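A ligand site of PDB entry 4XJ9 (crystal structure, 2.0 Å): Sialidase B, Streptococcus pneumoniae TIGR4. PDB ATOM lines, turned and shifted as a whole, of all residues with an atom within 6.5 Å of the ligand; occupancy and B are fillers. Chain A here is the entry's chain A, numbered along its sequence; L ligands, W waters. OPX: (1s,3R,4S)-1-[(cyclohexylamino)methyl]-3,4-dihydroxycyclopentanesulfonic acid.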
ATOM      1  N   LEU A 211      15.084  12.233  19.426  1.00  0.00           N
ATOM      2  CA  LEU A 211      13.648  12.246  19.719  1.00  0.00           C
ATOM      3  C   LEU A 211      12.914  11.897  18.433  1.00  0.00           C
ATOM      4  O   LEU A 211      13.333  12.294  17.344  1.00  0.00           O
ATOM      5  CB  LEU A 211      13.192  13.626  20.167  1.00  0.00           C
ATOM      6  CG  LEU A 211      13.552  14.114  21.576  1.00  0.00           C
ATOM      7  CD1 LEU A 211      13.158  15.577  21.743  1.00  0.00           C
ATOM      8  CD2 LEU A 211      12.860  13.258  22.597  1.00  0.00           C
ATOM      9  N   TYR A 212      11.820  11.163  18.545  1.00  0.00           N
ATOM     10  CA  TYR A 212      11.028  10.806  17.366  1.00  0.00           C
ATOM     11  C   TYR A 212       9.597  10.512  17.781  1.00  0.00           C
ATOM     12  O   TYR A 212       9.345   9.785  18.752  1.00  0.00           O
ATOM     13  CB  TYR A 212      11.640   9.587  16.687  1.00  0.00           C
ATOM     14  CG  TYR A 212      11.126   9.279  15.299  1.00  0.00           C
ATOM     15  CD1 TYR A 212      11.895   9.544  14.189  1.00  0.00           C
ATOM     16  CD2 TYR A 212       9.877   8.701  15.100  1.00  0.00           C
ATOM     17  CE1 TYR A 212      11.455   9.249  12.905  1.00  0.00           C
ATOM     18  CE2 TYR A 212       9.414   8.408  13.817  1.00  0.00           C
ATOM     19  CZ  TYR A 212      10.203   8.682  12.725  1.00  0.00           C
ATOM     20  OH  TYR A 212       9.773   8.393  11.450  1.00  0.00           O
ATOM     21  N   THR A 213       8.645  11.077  17.047  1.00  0.00           N
ATOM     22  CA  THR A 213       7.245  10.925  17.376  1.00  0.00           C
ATOM     23  C   THR A 213       6.643   9.782  16.560  1.00  0.00           C
ATOM     24  O   THR A 213       6.588   9.846  15.323  1.00  0.00           O
ATOM     25  CB  THR A 213       6.487  12.235  17.114  1.00  0.00           C
ATOM     26  OG1 THR A 213       7.048  13.283  17.908  1.00  0.00           O
ATOM     27  CG2 THR A 213       4.994  12.083  17.479  1.00  0.00           C
ATOM     28  N   LEU A 214       6.209   8.734  17.251  1.00  0.00           N
ATOM     29  CA  LEU A 214       5.656   7.546  16.591  1.00  0.00           C
ATOM     30  C   LEU A 214       4.185   7.769  16.242  1.00  0.00           C
ATOM     31  O   LEU A 214       3.532   8.642  16.819  1.00  0.00           O
ATOM     32  CB  LEU A 214       5.803   6.331  17.507  1.00  0.00           C
ATOM     33  CG  LEU A 214       7.222   6.041  18.003  1.00  0.00           C
ATOM     34  CD1 LEU A 214       7.237   4.879  18.979  1.00  0.00           C
ATOM     35  CD2 LEU A 214       8.121   5.747  16.805  1.00  0.00           C
ATOM     36  N   GLU A 294      10.510   5.205  12.272  1.00  0.00           N
ATOM     37  CA  GLU A 294       9.427   4.230  12.332  1.00  0.00           C
ATOM     38  C   GLU A 294       8.978   3.858  10.920  1.00  0.00           C
ATOM     39  O   GLU A 294       8.873   4.725  10.040  1.00  0.00           O
ATOM     40  CB  GLU A 294       8.240   4.724  13.159  1.00  0.00           C
ATOM     41  CG  GLU A 294       7.153   3.654  13.408  1.00  0.00           C
ATOM     42  CD  GLU A 294       6.019   4.147  14.303  1.00  0.00           C
ATOM     43  OE1 GLU A 294       5.358   5.144  13.934  1.00  0.00           O
ATOM     44  OE2 GLU A 294       5.778   3.536  15.366  1.00  0.00           O
ATOM     45  N   GLN A 456      17.187  11.468  13.678  1.00  0.00           N
ATOM     46  CA  GLN A 456      16.069  10.758  13.097  1.00  0.00           C
ATOM     47  C   GLN A 456      16.459  10.243  11.726  1.00  0.00           C
ATOM     48  O   GLN A 456      17.190  10.927  10.995  1.00  0.00           O
ATOM     49  CB  GLN A 456      14.870  11.707  12.934  1.00  0.00           C
ATOM     50  CG  GLN A 456      14.452  12.457  14.207  1.00  0.00           C
ATOM     51  CD  GLN A 456      13.228  13.330  13.966  1.00  0.00           C
ATOM     52  OE1 GLN A 456      12.830  13.582  12.812  1.00  0.00           O
ATOM     53  NE2 GLN A 456      12.604  13.796  15.046  1.00  0.00           N
ATOM     54  N   GLY A 457      15.989   9.057  11.386  1.00  0.00           N
ATOM     55  CA  GLY A 457      15.924   8.649   9.995  1.00  0.00           C
ATOM     56  C   GLY A 457      14.688   9.309   9.436  1.00  0.00           C
ATOM     57  O   GLY A 457      13.953   9.975  10.174  1.00  0.00           O
ATOM     58  N   LEU A 458      14.428   9.130   8.142  1.00  0.00           N
ATOM     59  CA  LEU A 458      13.283   9.784   7.516  1.00  0.00           C
ATOM     60  C   LEU A 458      12.386   8.744   6.895  1.00  0.00           C
ATOM     61  O   LEU A 458      12.841   7.945   6.095  1.00  0.00           O
ATOM     62  CB  LEU A 458      13.749  10.756   6.429  1.00  0.00           C
ATOM     63  CG  LEU A 458      12.658  11.425   5.595  1.00  0.00           C
ATOM     64  CD1 LEU A 458      11.761  12.254   6.489  1.00  0.00           C
ATOM     65  CD2 LEU A 458      13.278  12.307   4.513  1.00  0.00           C
ATOM     66  N   ALA A 459      11.117   8.756   7.310  1.00  0.00           N
ATOM     67  CA  ALA A 459      10.089   7.932   6.671  1.00  0.00           C
ATOM     68  C   ALA A 459       9.321   8.812   5.709  1.00  0.00           C
ATOM     69  O   ALA A 459       8.692   9.790   6.114  1.00  0.00           O
ATOM     70  CB  ALA A 459       9.127   7.362   7.712  1.00  0.00           C
ATOM     71  N   LEU A 460       9.366   8.465   4.433  1.00  0.00           N
ATOM     72  CA  LEU A 460       8.697   9.269   3.417  1.00  0.00           C
ATOM     73  C   LEU A 460       7.177   9.122   3.509  1.00  0.00           C
ATOM     74  O   LEU A 460       6.672   8.026   3.756  1.00  0.00           O
ATOM     75  CB  LEU A 460       9.217   8.914   2.031  1.00  0.00           C
ATOM     76  CG  LEU A 460      10.621   9.451   1.719  1.00  0.00           C
ATOM     77  CD1 LEU A 460      11.719   8.707   2.464  1.00  0.00           C
ATOM     78  CD2 LEU A 460      10.883   9.372   0.252  1.00  0.00           C
ATOM     79  N   LYS A 461       6.455  10.231   3.339  1.00  0.00           N
ATOM     80  CA  LYS A 461       5.012  10.281   3.526  1.00  0.00           C
ATOM     81  C   LYS A 461       4.210   9.367   2.603  1.00  0.00           C
ATOM     82  O   LYS A 461       3.285   8.675   3.062  1.00  0.00           O
ATOM     83  CB  LYS A 461       4.507  11.713   3.328  1.00  0.00           C
ATOM     84  CG  LYS A 461       5.045  12.695   4.338  1.00  0.00           C
ATOM     85  CD  LYS A 461       4.921  12.147   5.748  1.00  0.00           C
ATOM     86  CE  LYS A 461       5.362  13.188   6.765  1.00  0.00           C
ATOM     87  NZ  LYS A 461       4.469  14.385   6.784  1.00  0.00           N
ATOM     88  N   ALA A 557      16.553  18.878  12.701  1.00  0.00           N
ATOM     89  CA  ALA A 557      15.646  19.543  11.774  1.00  0.00           C
ATOM     90  C   ALA A 557      14.345  18.774  11.611  1.00  0.00           C
ATOM     91  O   ALA A 557      14.365  17.565  11.396  1.00  0.00           O
ATOM     92  CB  ALA A 557      16.313  19.708  10.413  1.00  0.00           C
ATOM     93  N   ILE A 558      13.222  19.493  11.685  1.00  0.00           N
ATOM     94  CA  ILE A 558      11.906  18.899  11.422  1.00  0.00           C
ATOM     95  C   ILE A 558      11.071  19.769  10.497  1.00  0.00           C
ATOM     96  O   ILE A 558      11.291  20.974  10.382  1.00  0.00           O
ATOM     97  CB  ILE A 558      11.100  18.678  12.710  1.00  0.00           C
ATOM     98  CG1 ILE A 558      10.865  20.021  13.414  1.00  0.00           C
ATOM     99  CG2 ILE A 558      11.786  17.661  13.628  1.00  0.00           C
ATOM    100  CD1 ILE A 558       9.878  19.968  14.563  1.00  0.00           C
ATOM    101  N   LYS A 559      10.100  19.129   9.843  1.00  0.00           N
ATOM    102  CA  LYS A 559       9.069  19.849   9.119  1.00  0.00           C
ATOM    103  C   LYS A 559       7.836  19.901  10.022  1.00  0.00           C
ATOM    104  O   LYS A 559       7.333  18.864  10.452  1.00  0.00           O
ATOM    105  CB  LYS A 559       8.735  19.106   7.822  1.00  0.00           C
ATOM    106  CG  LYS A 559       7.487  19.608   7.107  1.00  0.00           C
ATOM    107  CD  LYS A 559       7.815  20.563   5.991  1.00  0.00           C
ATOM    108  CE  LYS A 559       6.619  20.738   5.043  1.00  0.00           C
ATOM    109  NZ  LYS A 559       5.558  21.608   5.626  1.00  0.00           N
ATOM    110  N   SER A 561       3.983  20.308  11.188  1.00  0.00           N
ATOM    111  CA  SER A 561       2.793  19.767  10.552  1.00  0.00           C
ATOM    112  C   SER A 561       1.793  20.872  10.228  1.00  0.00           C
ATOM    113  O   SER A 561       0.935  20.705   9.356  1.00  0.00           O
ATOM    114  CB  SER A 561       2.127  18.722  11.461  1.00  0.00           C
ATOM    115  OG  SER A 561       1.446  19.358  12.526  1.00  0.00           O
ATOM    116  N   ILE A 618      15.010  17.451  18.211  1.00  0.00           N
ATOM    117  CA  ILE A 618      13.705  18.105  18.266  1.00  0.00           C
ATOM    118  C   ILE A 618      12.633  17.251  17.615  1.00  0.00           C
ATOM    119  O   ILE A 618      12.894  16.517  16.675  1.00  0.00           O
ATOM    120  CB  ILE A 618      13.686  19.497  17.618  1.00  0.00           C
ATOM    121  CG1 ILE A 618      14.251  19.462  16.206  1.00  0.00           C
ATOM    122  CG2 ILE A 618      14.450  20.518  18.485  1.00  0.00           C
ATOM    123  CD1 ILE A 618      14.252  20.826  15.540  1.00  0.00           C
ATOM    124  N   THR A 619      11.418  17.354  18.133  1.00  0.00           N
ATOM    125  CA  THR A 619      10.325  16.644  17.489  1.00  0.00           C
ATOM    126  C   THR A 619       9.017  17.349  17.760  1.00  0.00           C
ATOM    127  O   THR A 619       8.843  17.982  18.813  1.00  0.00           O
ATOM    128  CB  THR A 619      10.273  15.157  17.894  1.00  0.00           C
ATOM    129  OG1 THR A 619       9.482  14.430  16.949  1.00  0.00           O
ATOM    130  CG2 THR A 619       9.691  14.958  19.316  1.00  0.00           C
ATOM    131  N   GLU A 620       8.095  17.264  16.808  1.00  0.00           N
ATOM    132  CA  GLU A 620       6.780  17.827  17.021  1.00  0.00           C
ATOM    133  C   GLU A 620       6.002  16.823  17.849  1.00  0.00           C
ATOM    134  O   GLU A 620       5.802  15.691  17.422  1.00  0.00           O
ATOM    135  CB  GLU A 620       6.046  18.083  15.705  1.00  0.00           C
ATOM    136  CG  GLU A 620       4.648  18.720  15.912  1.00  0.00           C
ATOM    137  CD  GLU A 620       3.954  19.069  14.597  1.00  0.00           C
ATOM    138  OE1 GLU A 620       4.572  18.929  13.525  1.00  0.00           O
ATOM    139  OE2 GLU A 620       2.770  19.468  14.658  1.00  0.00           O
ATOM    140  N   LEU A 621       5.590  17.227  19.047  1.00  0.00           N
ATOM    141  CA  LEU A 621       4.767  16.371  19.894  1.00  0.00           C
ATOM    142  C   LEU A 621       3.383  16.221  19.267  1.00  0.00           C
ATOM    143  O   LEU A 621       2.977  17.051  18.453  1.00  0.00           O
ATOM    144  CB  LEU A 621       4.666  16.983  21.281  1.00  0.00           C
ATOM    145  CG  LEU A 621       6.063  17.251  21.858  1.00  0.00           C
ATOM    146  CD1 LEU A 621       5.970  17.935  23.192  1.00  0.00           C
ATOM    147  CD2 LEU A 621       6.834  15.969  21.972  1.00  0.00           C
ATOM    148  N   PRO A 622       2.641  15.166  19.634  1.00  0.00           N
ATOM    149  CA  PRO A 622       1.328  14.968  18.999  1.00  0.00           C
ATOM    150  C   PRO A 622       0.333  16.112  19.248  1.00  0.00           C
ATOM    151  O   PRO A 622      -0.616  16.270  18.479  1.00  0.00           O
ATOM    152  CB  PRO A 622       0.821  13.677  19.644  1.00  0.00           C
ATOM    153  CG  PRO A 622       2.071  12.941  20.084  1.00  0.00           C
ATOM    154  CD  PRO A 622       3.034  14.021  20.491  1.00  0.00           C
ATOM    155  N   ASN A 623       0.551  16.904  20.300  1.00  0.00           N
ATOM    156  CA  ASN A 623      -0.335  18.033  20.594  1.00  0.00           C
ATOM    157  C   ASN A 623       0.188  19.307  19.941  1.00  0.00           C
ATOM    158  O   ASN A 623      -0.249  20.407  20.272  1.00  0.00           O
ATOM    159  CB  ASN A 623      -0.454  18.231  22.103  1.00  0.00           C
ATOM    160  CG  ASN A 623       0.894  18.512  22.761  1.00  0.00           C
ATOM    161  OD1 ASN A 623       1.924  18.586  22.094  1.00  0.00           O
ATOM    162  ND2 ASN A 623       0.880  18.683  24.085  1.00  0.00           N
ATOM    163  N   HIS A 624       1.149  19.143  19.022  1.00  0.00           N
ATOM    164  CA  HIS A 624       1.744  20.243  18.241  1.00  0.00           C
ATOM    165  C   HIS A 624       2.709  21.155  18.991  1.00  0.00           C
ATOM    166  O   HIS A 624       3.193  22.143  18.429  1.00  0.00           O
ATOM    167  CB  HIS A 624       0.669  21.040  17.496  1.00  0.00           C
ATOM    168  CG  HIS A 624      -0.223  20.188  16.650  1.00  0.00           C
ATOM    169  ND1 HIS A 624       0.264  19.335  15.684  1.00  0.00           N
ATOM    170  CD2 HIS A 624      -1.572  20.040  16.629  1.00  0.00           C
ATOM    171  CE1 HIS A 624      -0.752  18.699  15.105  1.00  0.00           C
ATOM    172  NE2 HIS A 624      -1.869  19.119  15.665  1.00  0.00           N
HETATM  173  CAF OPX L   1       2.092  15.503  14.817  1.00  0.00           C
HETATM  174  CAG OPX L   1       1.652  14.728  13.603  1.00  0.00           C
HETATM  175  CAH OPX L   1       3.274  14.915  15.429  1.00  0.00           C
HETATM  176  CAI OPX L   1       2.740  14.393  12.655  1.00  0.00           C
HETATM  177  CAJ OPX L   1       4.347  14.689  14.442  1.00  0.00           C
HETATM  178  CAK OPX L   1       6.009  12.655  12.837  1.00  0.00           C
HETATM  179  CAL OPX L   1       8.112  13.769  12.058  1.00  0.00           C
HETATM  180  CAM OPX L   1       8.217  11.470  12.741  1.00  0.00           C
HETATM  181  CAO OPX L   1       9.495  13.394  12.357  1.00  0.00           C
HETATM  182  CAP OPX L   1       9.373  12.234  13.281  1.00  0.00           C
HETATM  183  CAQ OPX L   1       3.863  13.778  13.316  1.00  0.00           C
HETATM  184  CAR OPX L   1       7.307  12.510  12.087  1.00  0.00           C
HETATM  185  NAN OPX L   1       4.960  13.570  12.315  1.00  0.00           N
HETATM  186  OAA OPX L   1       5.951  12.984   9.789  1.00  0.00           O
HETATM  187  OAB OPX L   1       8.094  11.951   9.641  1.00  0.00           O
HETATM  188  OAC OPX L   1      10.165  14.458  12.959  1.00  0.00           O
HETATM  189  OAD OPX L   1       8.951  12.669  14.495  1.00  0.00           O
HETATM  190  OAE OPX L   1       6.273  10.599  10.472  1.00  0.00           O
HETATM  191  SAS OPX L   1       6.907  12.015  10.428  1.00  0.00           S
HETATM  192  O   HOH W   1       3.597  11.806  10.524  1.00  0.00           O
HETATM  193  O   HOH W   2      10.276  10.436   9.521  1.00  0.00           O
HETATM  194  O   HOH W   3       5.277  15.873  10.984  1.00  0.00           O
HETATM  195  O   HOH W   4       4.452   9.311   7.981  1.00  0.00           O
HETATM  196  O   HOH W   5       8.623  16.316  14.128  1.00  0.00           O
HETATM  197  O   HOH W   6       5.303   8.790  13.165  1.00  0.00           O
HETATM  198  O   HOH W   7      10.067  16.328  10.376  1.00  0.00           O
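The side-chain amide oxygen (OE1) of Gln 456 lies within hydrogen-bond range of an oxygen (OAC) of the ligand (2.8 Å). The backbone NH of Thr 213 lies within hydrogen-bond range of an oxygen (OAD) of the ligand (3.0 Å). The side-chain hydroxyl (OG1) of Thr 619 lies within hydrogen-bond range of an oxygen (OAD) of the ligand (3.1 Å). An oxygen (OAA) of the ligand lies within salt-bridge range of the side-chain amino group (NZ) of Lys 461.
O of Ile 618 lies within hydrogen-bond range of NE2 of Gln 456. The backbone carbonyl oxygen (O) of Leu 211 sits at hydrogen-bond distance from the side-chain amide nitrogen (NE2) of Gln 456, at 2.8 Å. The side-chain hydroxyl of Thr 213 sits at hydrogen-bond distance from the side-chain hydroxyl of Thr 619. OG1 of Thr 213 is in hydrogen-bond range of O of Glu 620, 2.8 Å away. The side-chain carboxylate (OE2) of Glu 620 is in hydrogen-bond range of a ring nitrogen (ND1) of His 624, at 2.7 Å. The side-chain carboxylate of Glu 620 lies within hydrogen-bond range of the side-chain hydroxyl of Ser 561, 2.5 Å away. The side-chain hydroxyl (OH) of Tyr 212 sits at hydrogen-bond distance from the backbone NH (N) of Glu 294, at 3.4 Å.
Residues that only touch the ligand: Tyr 212 (3.4 Å), Ile 558 (3.7 Å), Glu 620 (3.3 Å) and Leu 621 (3.7 Å). Hydrophobic or aromatic side chains within 4 Å of the ligand: Tyr 212 and Ile 558. Of the 22 residues printed, 8 come within 4 Å of the ligand. The nearest printed residue that does not touch the ligand is Pro 622 (4.1 Å).
Water W2 lies within hydrogen-bond range of an oxygen (OAB) of the ligand, the side-chain hydroxyl of Tyr 212 and the backbone NH of Ala 459. Water W5 bridges OAC of the ligand (2.7 Å) and N of Glu 620 (2.9 Å). Water W7 bridges the backbone NH of Lys 559 and an oxygen (OAC) of the ligand. Water W6 lies within hydrogen-bond range of the backbone carbonyl oxygen of Thr 213 (2.7 Å) and an oxygen (OAE) of the ligand (3.4 Å).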
